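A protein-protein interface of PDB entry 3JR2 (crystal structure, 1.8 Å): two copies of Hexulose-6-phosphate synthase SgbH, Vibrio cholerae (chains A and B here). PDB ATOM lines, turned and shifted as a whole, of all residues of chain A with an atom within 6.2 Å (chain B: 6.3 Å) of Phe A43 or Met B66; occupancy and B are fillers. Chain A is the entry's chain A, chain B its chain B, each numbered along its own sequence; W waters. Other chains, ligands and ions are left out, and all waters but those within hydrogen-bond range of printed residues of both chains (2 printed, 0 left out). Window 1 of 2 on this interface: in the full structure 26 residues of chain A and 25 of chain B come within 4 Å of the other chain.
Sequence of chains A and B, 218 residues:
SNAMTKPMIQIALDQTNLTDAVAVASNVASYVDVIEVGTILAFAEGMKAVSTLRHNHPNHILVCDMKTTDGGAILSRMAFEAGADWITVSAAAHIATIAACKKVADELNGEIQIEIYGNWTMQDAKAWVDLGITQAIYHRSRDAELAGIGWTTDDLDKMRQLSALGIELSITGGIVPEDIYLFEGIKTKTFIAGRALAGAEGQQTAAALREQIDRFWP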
ATOM      1  N   GLY A  38     -12.107 -19.889  -6.578  1.00  0.00           N
ATOM      2  CA  GLY A  38     -12.475 -18.724  -7.377  1.00  0.00           C
ATOM      3  C   GLY A  38     -11.271 -17.989  -7.943  1.00  0.00           C
ATOM      4  O   GLY A  38     -10.135 -18.183  -7.492  1.00  0.00           O
ATOM      5  N   THR A  39     -11.520 -17.128  -8.935  1.00  0.00           N
ATOM      6  CA  THR A  39     -10.468 -16.403  -9.589  1.00  0.00           C
ATOM      7  C   THR A  39      -9.695 -15.545  -8.593  1.00  0.00           C
ATOM      8  O   THR A  39      -8.492 -15.450  -8.681  1.00  0.00           O
ATOM      9  CB  THR A  39     -11.075 -15.521 -10.722  1.00  0.00           C
ATOM     10  OG1 THR A  39     -12.018 -16.313 -11.473  1.00  0.00           O
ATOM     11  CG2 THR A  39      -9.955 -14.985 -11.622  1.00  0.00           C
ATOM     12  N   ILE A  40     -10.363 -14.974  -7.586  1.00  0.00           N
ATOM     13  CA  ILE A  40      -9.680 -14.170  -6.573  1.00  0.00           C
ATOM     14  C   ILE A  40      -8.659 -15.000  -5.778  1.00  0.00           C
ATOM     15  O   ILE A  40      -7.539 -14.591  -5.548  1.00  0.00           O
ATOM     16  CB  ILE A  40     -10.718 -13.423  -5.652  1.00  0.00           C
ATOM     17  CG1 ILE A  40     -11.468 -12.373  -6.456  1.00  0.00           C
ATOM     18  CG2 ILE A  40     -10.053 -12.864  -4.368  1.00  0.00           C
ATOM     19  CD1 ILE A  40     -12.788 -11.948  -5.756  1.00  0.00           C
ATOM     20  N   LEU A  41      -9.039 -16.190  -5.374  1.00  0.00           N
ATOM     21  CA  LEU A  41      -8.191 -17.039  -4.563  1.00  0.00           C
ATOM     22  C   LEU A  41      -7.043 -17.546  -5.441  1.00  0.00           C
ATOM     23  O   LEU A  41      -5.909 -17.633  -5.002  1.00  0.00           O
ATOM     24  CB  LEU A  41      -8.974 -18.252  -4.058  1.00  0.00           C
ATOM     25  CG  LEU A  41      -8.205 -19.288  -3.215  1.00  0.00           C
ATOM     26  CD1 LEU A  41      -7.412 -18.663  -2.010  1.00  0.00           C
ATOM     27  CD2 LEU A  41      -9.147 -20.352  -2.676  1.00  0.00           C
ATOM     28  N   ALA A  42      -7.372 -17.892  -6.688  1.00  0.00           N
ATOM     29  CA  ALA A  42      -6.393 -18.345  -7.676  1.00  0.00           C
ATOM     30  C   ALA A  42      -5.311 -17.291  -7.967  1.00  0.00           C
ATOM     31  O   ALA A  42      -4.123 -17.601  -8.010  1.00  0.00           O
ATOM     32  CB  ALA A  42      -7.055 -18.805  -8.930  1.00  0.00           C
ATOM     33  N   PHE A  43      -5.691 -16.053  -8.184  1.00  0.00           N
ATOM     34  CA  PHE A  43      -4.669 -14.998  -8.270  1.00  0.00           C
ATOM     35  C   PHE A  43      -3.982 -14.657  -6.943  1.00  0.00           C
ATOM     36  O   PHE A  43      -2.835 -14.280  -6.940  1.00  0.00           O
ATOM     37  CB  PHE A  43      -5.209 -13.728  -8.870  1.00  0.00           C
ATOM     38  CG  PHE A  43      -5.328 -13.761 -10.377  1.00  0.00           C
ATOM     39  CD1 PHE A  43      -4.270 -14.097 -11.181  1.00  0.00           C
ATOM     40  CD2 PHE A  43      -6.551 -13.444 -10.985  1.00  0.00           C
ATOM     41  CE1 PHE A  43      -4.424 -14.115 -12.589  1.00  0.00           C
ATOM     42  CE2 PHE A  43      -6.697 -13.451 -12.351  1.00  0.00           C
ATOM     43  CZ  PHE A  43      -5.626 -13.795 -13.156  1.00  0.00           C
ATOM     44  N   ALA A  44      -4.660 -14.800  -5.805  1.00  0.00           N
ATOM     45  CA  ALA A  44      -4.003 -14.454  -4.561  1.00  0.00           C
ATOM     46  C   ALA A  44      -2.861 -15.403  -4.276  1.00  0.00           C
ATOM     47  O   ALA A  44      -1.759 -14.980  -3.889  1.00  0.00           O
ATOM     48  CB  ALA A  44      -4.996 -14.426  -3.379  1.00  0.00           C
ATOM     49  N   GLU A  45      -3.136 -16.703  -4.467  1.00  0.00           N
ATOM     50  CA  GLU A  45      -2.258 -17.747  -4.035  1.00  0.00           C
ATOM     51  C   GLU A  45      -1.641 -18.627  -5.100  1.00  0.00           C
ATOM     52  O   GLU A  45      -0.695 -19.364  -4.825  1.00  0.00           O
ATOM     53  CB  GLU A  45      -3.065 -18.618  -3.087  1.00  0.00           C
ATOM     54  CG  GLU A  45      -3.482 -17.828  -1.859  1.00  0.00           C
ATOM     55  CD  GLU A  45      -2.402 -17.661  -0.758  1.00  0.00           C
ATOM     56  OE1 GLU A  45      -1.238 -18.061  -0.956  1.00  0.00           O
ATOM     57  OE2 GLU A  45      -2.730 -17.142   0.340  1.00  0.00           O
ATOM     58  N   GLY A  46      -2.183 -18.588  -6.312  1.00  0.00           N
ATOM     59  CA  GLY A  46      -1.737 -19.428  -7.372  1.00  0.00           C
ATOM     60  C   GLY A  46      -2.201 -20.862  -7.197  1.00  0.00           C
ATOM     61  O   GLY A  46      -3.047 -21.153  -6.383  1.00  0.00           O
ATOM     62  N   MET A  66     -10.314 -20.019 -13.595  1.00  0.00           N
ATOM     63  CA  MET A  66      -9.355 -19.090 -14.132  1.00  0.00           C
ATOM     64  C   MET A  66      -9.918 -18.093 -15.169  1.00  0.00           C
ATOM     65  O   MET A  66      -9.221 -17.119 -15.521  1.00  0.00           O
ATOM     66  CB  MET A  66      -8.242 -19.877 -14.808  1.00  0.00           C
ATOM     67  CG  MET A  66      -7.389 -20.606 -13.778  1.00  0.00           C
ATOM     68  SD  MET A  66      -5.975 -21.615 -14.673  1.00  0.00           S
ATOM     69  CE  MET A  66      -7.072 -22.839 -15.643  1.00  0.00           C
ATOM     70  N   VAL B  37       4.066  -9.223 -15.285  1.00  0.00           N
ATOM     71  CA  VAL B  37       3.644 -10.521 -14.754  1.00  0.00           C
ATOM     72  C   VAL B  37       2.460 -10.995 -15.596  1.00  0.00           C
ATOM     73  O   VAL B  37       1.349 -10.529 -15.440  1.00  0.00           O
ATOM     74  CB  VAL B  37       3.334 -10.505 -13.248  1.00  0.00           C
ATOM     75  CG1 VAL B  37       2.844 -11.908 -12.759  1.00  0.00           C
ATOM     76  CG2 VAL B  37       4.514 -10.011 -12.428  1.00  0.00           C
ATOM     77  N   GLY B  38       2.749 -11.873 -16.526  1.00  0.00           N
ATOM     78  CA  GLY B  38       1.769 -12.454 -17.401  1.00  0.00           C
ATOM     79  C   GLY B  38       0.798 -13.313 -16.628  1.00  0.00           C
ATOM     80  O   GLY B  38       1.101 -13.817 -15.532  1.00  0.00           O
ATOM     81  N   THR B  39      -0.354 -13.594 -17.252  1.00  0.00           N
ATOM     82  CA  THR B  39      -1.379 -14.365 -16.599  1.00  0.00           C
ATOM     83  C   THR B  39      -0.887 -15.735 -16.157  1.00  0.00           C
ATOM     84  O   THR B  39      -1.290 -16.241 -15.106  1.00  0.00           O
ATOM     85  CB  THR B  39      -2.604 -14.499 -17.561  1.00  0.00           C
ATOM     86  OG1 THR B  39      -2.843 -13.246 -18.199  1.00  0.00           O
ATOM     87  CG2 THR B  39      -3.882 -14.914 -16.827  1.00  0.00           C
ATOM     88  N   ALA B  42       1.125 -15.309 -12.997  1.00  0.00           N
ATOM     89  CA  ALA B  42       0.172 -14.878 -11.963  1.00  0.00           C
ATOM     90  C   ALA B  42      -0.611 -16.079 -11.400  1.00  0.00           C
ATOM     91  O   ALA B  42      -0.741 -16.234 -10.158  1.00  0.00           O
ATOM     92  CB  ALA B  42      -0.769 -13.813 -12.478  1.00  0.00           C
ATOM     93  N   PHE B  43      -1.115 -16.918 -12.285  1.00  0.00           N
ATOM     94  CA  PHE B  43      -1.827 -18.153 -11.828  1.00  0.00           C
ATOM     95  C   PHE B  43      -0.891 -19.214 -11.263  1.00  0.00           C
ATOM     96  O   PHE B  43      -1.250 -19.981 -10.391  1.00  0.00           O
ATOM     97  CB  PHE B  43      -2.725 -18.776 -12.898  1.00  0.00           C
ATOM     98  CG  PHE B  43      -4.051 -18.090 -13.063  1.00  0.00           C
ATOM     99  CD1 PHE B  43      -4.865 -17.824 -11.972  1.00  0.00           C
ATOM    100  CD2 PHE B  43      -4.492 -17.710 -14.307  1.00  0.00           C
ATOM    101  CE1 PHE B  43      -6.105 -17.175 -12.148  1.00  0.00           C
ATOM    102  CE2 PHE B  43      -5.757 -17.083 -14.490  1.00  0.00           C
ATOM    103  CZ  PHE B  43      -6.527 -16.803 -13.414  1.00  0.00           C
ATOM    104  N   GLU B  45       1.871 -18.667  -9.511  1.00  0.00           N
ATOM    105  CA  GLU B  45       2.573 -18.287  -8.298  1.00  0.00           C
ATOM    106  C   GLU B  45       1.761 -17.410  -7.355  1.00  0.00           C
ATOM    107  O   GLU B  45       2.109 -17.302  -6.189  1.00  0.00           O
ATOM    108  CB  GLU B  45       3.927 -17.602  -8.631  1.00  0.00           C
ATOM    109  CG  GLU B  45       4.928 -18.531  -9.350  1.00  0.00           C
ATOM    110  CD  GLU B  45       5.607 -19.557  -8.440  1.00  0.00           C
ATOM    111  OE1 GLU B  45       5.258 -19.590  -7.293  1.00  0.00           O
ATOM    112  OE2 GLU B  45       6.531 -20.277  -8.880  1.00  0.00           O
ATOM    113  N   GLY B  46       0.723 -16.772  -7.858  1.00  0.00           N
ATOM    114  CA  GLY B  46      -0.049 -15.818  -7.107  1.00  0.00           C
ATOM    115  C   GLY B  46       0.643 -14.477  -7.017  1.00  0.00           C
ATOM    116  O   GLY B  46       1.669 -14.189  -7.687  1.00  0.00           O
ATOM    117  N   MET B  47       0.090 -13.630  -6.168  1.00  0.00           N
ATOM    118  CA  MET B  47       0.590 -12.264  -6.020  1.00  0.00           C
ATOM    119  C   MET B  47       2.043 -12.092  -5.565  1.00  0.00           C
ATOM    120  O   MET B  47       2.643 -11.053  -5.806  1.00  0.00           O
ATOM    121  CB  MET B  47      -0.349 -11.449  -5.124  1.00  0.00           C
ATOM    122  CG  MET B  47      -1.633 -11.134  -5.734  1.00  0.00           C
ATOM    123  SD  MET B  47      -1.652 -10.105  -7.395  1.00  0.00           S
ATOM    124  CE  MET B  47      -1.581 -11.625  -8.640  1.00  0.00           C
ATOM    125  N   LYS B  48       2.626 -13.092  -4.916  1.00  0.00           N
ATOM    126  CA  LYS B  48       4.010 -13.021  -4.574  1.00  0.00           C
ATOM    127  C   LYS B  48       4.881 -12.797  -5.831  1.00  0.00           C
ATOM    128  O   LYS B  48       5.956 -12.200  -5.729  1.00  0.00           O
ATOM    129  CB  LYS B  48       4.467 -14.269  -3.790  1.00  0.00           C
ATOM    130  CG  LYS B  48       4.563 -15.513  -4.587  1.00  0.00           C
ATOM    131  CD  LYS B  48       5.273 -16.604  -3.811  1.00  0.00           C
ATOM    132  CE  LYS B  48       5.332 -17.970  -4.539  1.00  0.00           C
ATOM    133  NZ  LYS B  48       3.917 -18.512  -4.699  1.00  0.00           N
ATOM    134  N   CYS B  64       0.498  -6.174 -13.936  1.00  0.00           N
ATOM    135  CA  CYS B  64      -0.115  -7.456 -13.521  1.00  0.00           C
ATOM    136  C   CYS B  64      -1.227  -7.793 -14.537  1.00  0.00           C
ATOM    137  O   CYS B  64      -2.280  -7.137 -14.545  1.00  0.00           O
ATOM    138  CB  CYS B  64      -0.694  -7.386 -12.102  1.00  0.00           C
ATOM    139  SG  CYS B  64      -1.234  -9.034 -11.566  1.00  0.00           S
ATOM    140  N   ASP B  65      -0.982  -8.809 -15.376  1.00  0.00           N
ATOM    141  CA  ASP B  65      -1.878  -9.208 -16.465  1.00  0.00           C
ATOM    142  C   ASP B  65      -2.899 -10.238 -16.019  1.00  0.00           C
ATOM    143  O   ASP B  65      -2.647 -11.429 -16.081  1.00  0.00           O
ATOM    144  CB  ASP B  65      -1.042  -9.786 -17.609  1.00  0.00           C
ATOM    145  CG  ASP B  65      -1.851 -10.058 -18.851  1.00  0.00           C
ATOM    146  OD1 ASP B  65      -3.050  -9.743 -18.866  1.00  0.00           O
ATOM    147  OD2 ASP B  65      -1.277 -10.628 -19.798  1.00  0.00           O
ATOM    148  N   MET B  66      -3.989  -9.761 -15.415  1.00  0.00           N
ATOM    149  CA  MET B  66      -5.005 -10.625 -14.903  1.00  0.00           C
ATOM    150  C   MET B  66      -6.123 -10.904 -15.912  1.00  0.00           C
ATOM    151  O   MET B  66      -6.855 -11.896 -15.724  1.00  0.00           O
ATOM    152  CB  MET B  66      -5.607 -10.017 -13.599  1.00  0.00           C
ATOM    153  CG  MET B  66      -4.584 -10.128 -12.504  1.00  0.00           C
ATOM    154  SD  MET B  66      -5.312  -9.428 -10.824  1.00  0.00           S
ATOM    155  CE  MET B  66      -5.593  -7.711 -11.425  1.00  0.00           C
ATOM    156  N   LYS B  67      -6.256 -10.065 -16.944  1.00  0.00           N
ATOM    157  CA  LYS B  67      -7.382 -10.152 -17.904  1.00  0.00           C
ATOM    158  C   LYS B  67      -8.733 -10.237 -17.137  1.00  0.00           C
ATOM    159  O   LYS B  67      -9.588 -11.077 -17.417  1.00  0.00           O
ATOM    160  CB  LYS B  67      -7.222 -11.320 -18.864  1.00  0.00           C
ATOM    161  CG  LYS B  67      -5.949 -11.143 -19.713  1.00  0.00           C
ATOM    162  CD  LYS B  67      -5.822 -12.232 -20.762  1.00  0.00           C
ATOM    163  CE  LYS B  67      -4.501 -12.283 -21.450  1.00  0.00           C
ATOM    164  NZ  LYS B  67      -3.344 -12.177 -20.575  1.00  0.00           N
ATOM    165  N   THR B  68      -8.845  -9.358 -16.175  1.00  0.00           N
ATOM    166  CA  THR B  68      -9.914  -9.378 -15.144  1.00  0.00           C
ATOM    167  C   THR B  68     -11.227  -9.396 -15.870  1.00  0.00           C
ATOM    168  O   THR B  68     -11.436  -8.562 -16.720  1.00  0.00           O
ATOM    169  CB  THR B  68      -9.839  -8.081 -14.281  1.00  0.00           C
ATOM    170  OG1 THR B  68      -8.499  -7.972 -13.763  1.00  0.00           O
ATOM    171  CG2 THR B  68     -10.823  -8.172 -13.137  1.00  0.00           C
ATOM    172  N   THR B  69     -12.125 -10.312 -15.509  1.00  0.00           N
ATOM    173  CA  THR B  69     -13.390 -10.469 -16.224  1.00  0.00           C
ATOM    174  C   THR B  69     -14.557 -10.205 -15.267  1.00  0.00           C
ATOM    175  O   THR B  69     -15.637  -9.834 -15.699  1.00  0.00           O
ATOM    176  CB  THR B  69     -13.467 -11.855 -16.884  1.00  0.00           C
ATOM    177  OG1 THR B  69     -12.415 -11.949 -17.841  1.00  0.00           O
ATOM    178  CG2 THR B  69     -14.812 -12.079 -17.597  1.00  0.00           C
ATOM    179  N   LEU B  75      -9.876  -7.766  -7.202  1.00  0.00           N
ATOM    180  CA  LEU B  75      -8.665  -8.144  -7.963  1.00  0.00           C
ATOM    181  C   LEU B  75      -7.745  -6.956  -8.223  1.00  0.00           C
ATOM    182  O   LEU B  75      -6.529  -7.068  -8.074  1.00  0.00           O
ATOM    183  CB  LEU B  75      -9.073  -8.835  -9.281  1.00  0.00           C
ATOM    184  CG  LEU B  75      -9.456 -10.321  -9.206  1.00  0.00           C
ATOM    185  CD1 LEU B  75      -9.870 -10.786 -10.633  1.00  0.00           C
ATOM    186  CD2 LEU B  75      -8.348 -11.212  -8.685  1.00  0.00           C
ATOM    187  N   SER B  76      -8.337  -5.831  -8.622  1.00  0.00           N
ATOM    188  CA  SER B  76      -7.594  -4.642  -8.848  1.00  0.00           C
ATOM    189  C   SER B  76      -6.850  -4.191  -7.599  1.00  0.00           C
ATOM    190  O   SER B  76      -5.650  -3.917  -7.639  1.00  0.00           O
ATOM    191  CB  SER B  76      -8.549  -3.550  -9.270  1.00  0.00           C
ATOM    192  OG  SER B  76      -9.029  -3.840 -10.561  1.00  0.00           O
ATOM    193  N   MET B  78      -5.965  -6.040  -5.032  1.00  0.00           N
ATOM    194  CA  MET B  78      -4.953  -7.001  -4.667  1.00  0.00           C
ATOM    195  C   MET B  78      -3.661  -6.760  -5.487  1.00  0.00           C
ATOM    196  O   MET B  78      -2.557  -6.771  -4.958  1.00  0.00           O
ATOM    197  CB  MET B  78      -5.536  -8.419  -4.820  1.00  0.00           C
ATOM    198  CG  MET B  78      -4.569  -9.489  -4.986  1.00  0.00           C
ATOM    199  SD  MET B  78      -5.538 -11.151  -5.465  1.00  0.00           S
ATOM    200  CE  MET B  78      -7.224 -10.606  -4.576  1.00  0.00           C
ATOM    201  N   ALA B  79      -3.810  -6.496  -6.786  1.00  0.00           N
ATOM    202  CA  ALA B  79      -2.669  -6.305  -7.683  1.00  0.00           C
ATOM    203  C   ALA B  79      -1.912  -5.005  -7.393  1.00  0.00           C
ATOM    204  O   ALA B  79      -0.686  -4.982  -7.307  1.00  0.00           O
ATOM    205  CB  ALA B  79      -3.161  -6.311  -9.199  1.00  0.00           C
ATOM    206  N   ILE B  87      -2.658  -2.634 -14.469  1.00  0.00           N
ATOM    207  CA  ILE B  87      -3.328  -3.974 -14.462  1.00  0.00           C
ATOM    208  C   ILE B  87      -4.201  -4.110 -15.697  1.00  0.00           C
ATOM    209  O   ILE B  87      -4.626  -3.097 -16.277  1.00  0.00           O
ATOM    210  CB  ILE B  87      -4.113  -4.242 -13.220  1.00  0.00           C
ATOM    211  CG1 ILE B  87      -5.323  -3.307 -13.131  1.00  0.00           C
ATOM    212  CG2 ILE B  87      -3.240  -4.080 -11.973  1.00  0.00           C
ATOM    213  CD1 ILE B  87      -6.240  -3.700 -11.960  1.00  0.00           C
ATOM    214  N   THR B  88      -4.403  -5.346 -16.148  1.00  0.00           N
ATOM    215  CA  THR B  88      -5.232  -5.559 -17.323  1.00  0.00           C
ATOM    216  C   THR B  88      -6.639  -6.107 -16.955  1.00  0.00           C
ATOM    217  O   THR B  88      -6.866  -6.787 -15.944  1.00  0.00           O
ATOM    218  CB  THR B  88      -4.541  -6.495 -18.303  1.00  0.00           C
ATOM    219  OG1 THR B  88      -4.496  -7.804 -17.749  1.00  0.00           O
ATOM    220  CG2 THR B  88      -3.103  -5.981 -18.584  1.00  0.00           C
ATOM    221  N   VAL B  89      -7.583  -5.699 -17.764  1.00  0.00           N
ATOM    222  CA  VAL B  89      -8.989  -6.061 -17.616  1.00  0.00           C
ATOM    223  C   VAL B  89      -9.493  -6.489 -18.965  1.00  0.00           C
ATOM    224  O   VAL B  89      -9.249  -5.813 -19.982  1.00  0.00           O
ATOM    225  CB  VAL B  89      -9.752  -4.826 -17.116  1.00  0.00           C
ATOM    226  CG1 VAL B  89     -11.324  -5.103 -16.984  1.00  0.00           C
ATOM    227  CG2 VAL B  89      -9.145  -4.323 -15.783  1.00  0.00           C
ATOM    228  N   SER B  90     -10.192  -7.629 -19.005  1.00  0.00           N
ATOM    229  CA  SER B  90     -10.713  -8.137 -20.259  1.00  0.00           C
ATOM    230  C   SER B  90     -11.772  -7.185 -20.851  1.00  0.00           C
ATOM    231  O   SER B  90     -12.606  -6.657 -20.135  1.00  0.00           O
ATOM    232  CB  SER B  90     -11.365  -9.508 -19.995  1.00  0.00           C
ATOM    233  OG  SER B  90     -11.858 -10.017 -21.219  1.00  0.00           O
HETATM  234  O   HOH W   1       1.109 -15.345  -3.688  1.00  0.00           O
HETATM  235  O   HOH W   2       1.421 -17.985  -3.190  1.00  0.00           O
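Of the 23 printed residues of chain B, 8 touch a printed residue of chain A. Hydrophobic or aromatic side chains of chain B that line the printed part of chain A: Ala B42, Phe B43, Met B47, Met B66, Leu B75 and Met B78. Printed residues of chain A that touch a printed residue of chain B: Ile A40, Ala A42, Phe A43, Ala A44, Glu A45, Gly A46 and Met A66. Among the printed residues, 17 pairs touch across the chains. Among the printed residues, no Asp or Glu carboxylate lies within 4 Å of a Lys or Arg side-chain nitrogen of the other chain.
Of the printed residues of chain B, Phe A43 touches Ala B42 (3.7 Å), Phe B43 (3.2 Å), Gly B46 (3.2 Å), Met B47 (3.1 Å), Met B66 (3.4 Å) and Leu B75 (3.7 Å). Gly B38 touches none of the printed residues of chain A. Of the printed residues of chain A, Phe B43 touches Ala A42, Phe A43, Gly A46 and Met A66. Printed residues of chain A within 4 Å of Met B47: Phe A43 and Ala A44. Of chain A, only Phe A43 comes within 4 Å of Met B66. Thr B69 touches none of the printed residues of chain A. Of the printed residues of chain A, Leu B75 touches Ile A40 (3.9 Å) and Phe A43 (3.7 Å). The nearest printed residue of chain A that does not touch Ala B42 is Ala A42 (4.2 Å).
Ile A40 touches Leu B75. Met B78 touches Ile A40. CB of Ala A42 touches CE1 of Phe B43, 3.7 Å away. Phe B43 touches Phe A43 (CZ to CZ, 3.2 Å). Phe A43 touches Gly B46 (O to CA, 3.2 Å). Leu B75 touches Phe A43 (CD2 to CD2, 3.7 Å). Ala A44 touches Gly B46 (O to CA, 3.7 Å). Glu A45 touches Glu B45. Gly B46 touches Glu A45. Met A66 touches Phe B43.
The backbone carbonyl oxygen (O) of Phe A43 is in hydrogen-bond range of the backbone NH (N) of Met B47. The backbone NH (N) of Ala A44 lies close to the side-chain sulfur (SD) of Met B78, 3.8 Å away. The backbone carbonyl oxygen of Ala A44 sits at hydrogen-bond distance from the backbone NH of Met B47 (3.2 Å).
Water W1 lies within hydrogen-bond range of O of Ala A44 (2.9 Å), N of Lys B48 (3.0 Å), N of Met B47 (3.2 Å) and O of Glu B45 (3.3 Å). Water W2 lies within hydrogen-bond range of the side-chain amino group of Lys B48 (3.0 Å), the backbone carbonyl oxygen of Glu A45 (3.0 Å) and the backbone carbonyl oxygen of Glu B45 (3.2 Å).
Ala A42 touches Phe B43, and with the chains exchanged Phe A43 touches Ala B42. Phe B43 touches its own counterpart, Phe A43. Phe A43 touches Met B66, and with the chains exchanged Met A66 touches Phe B43. Gly B46 touches its own counterpart, Gly A46. Positions printed for both chains: 38, 39, 42, 43, 45, 46 and 66.
N of Met B66 is in hydrogen-bond range of OG1 of Thr B88 (3.1 Å). OE1 of Glu B45 lies within salt-bridge range of NZ of Lys B48 (3.1 Å).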
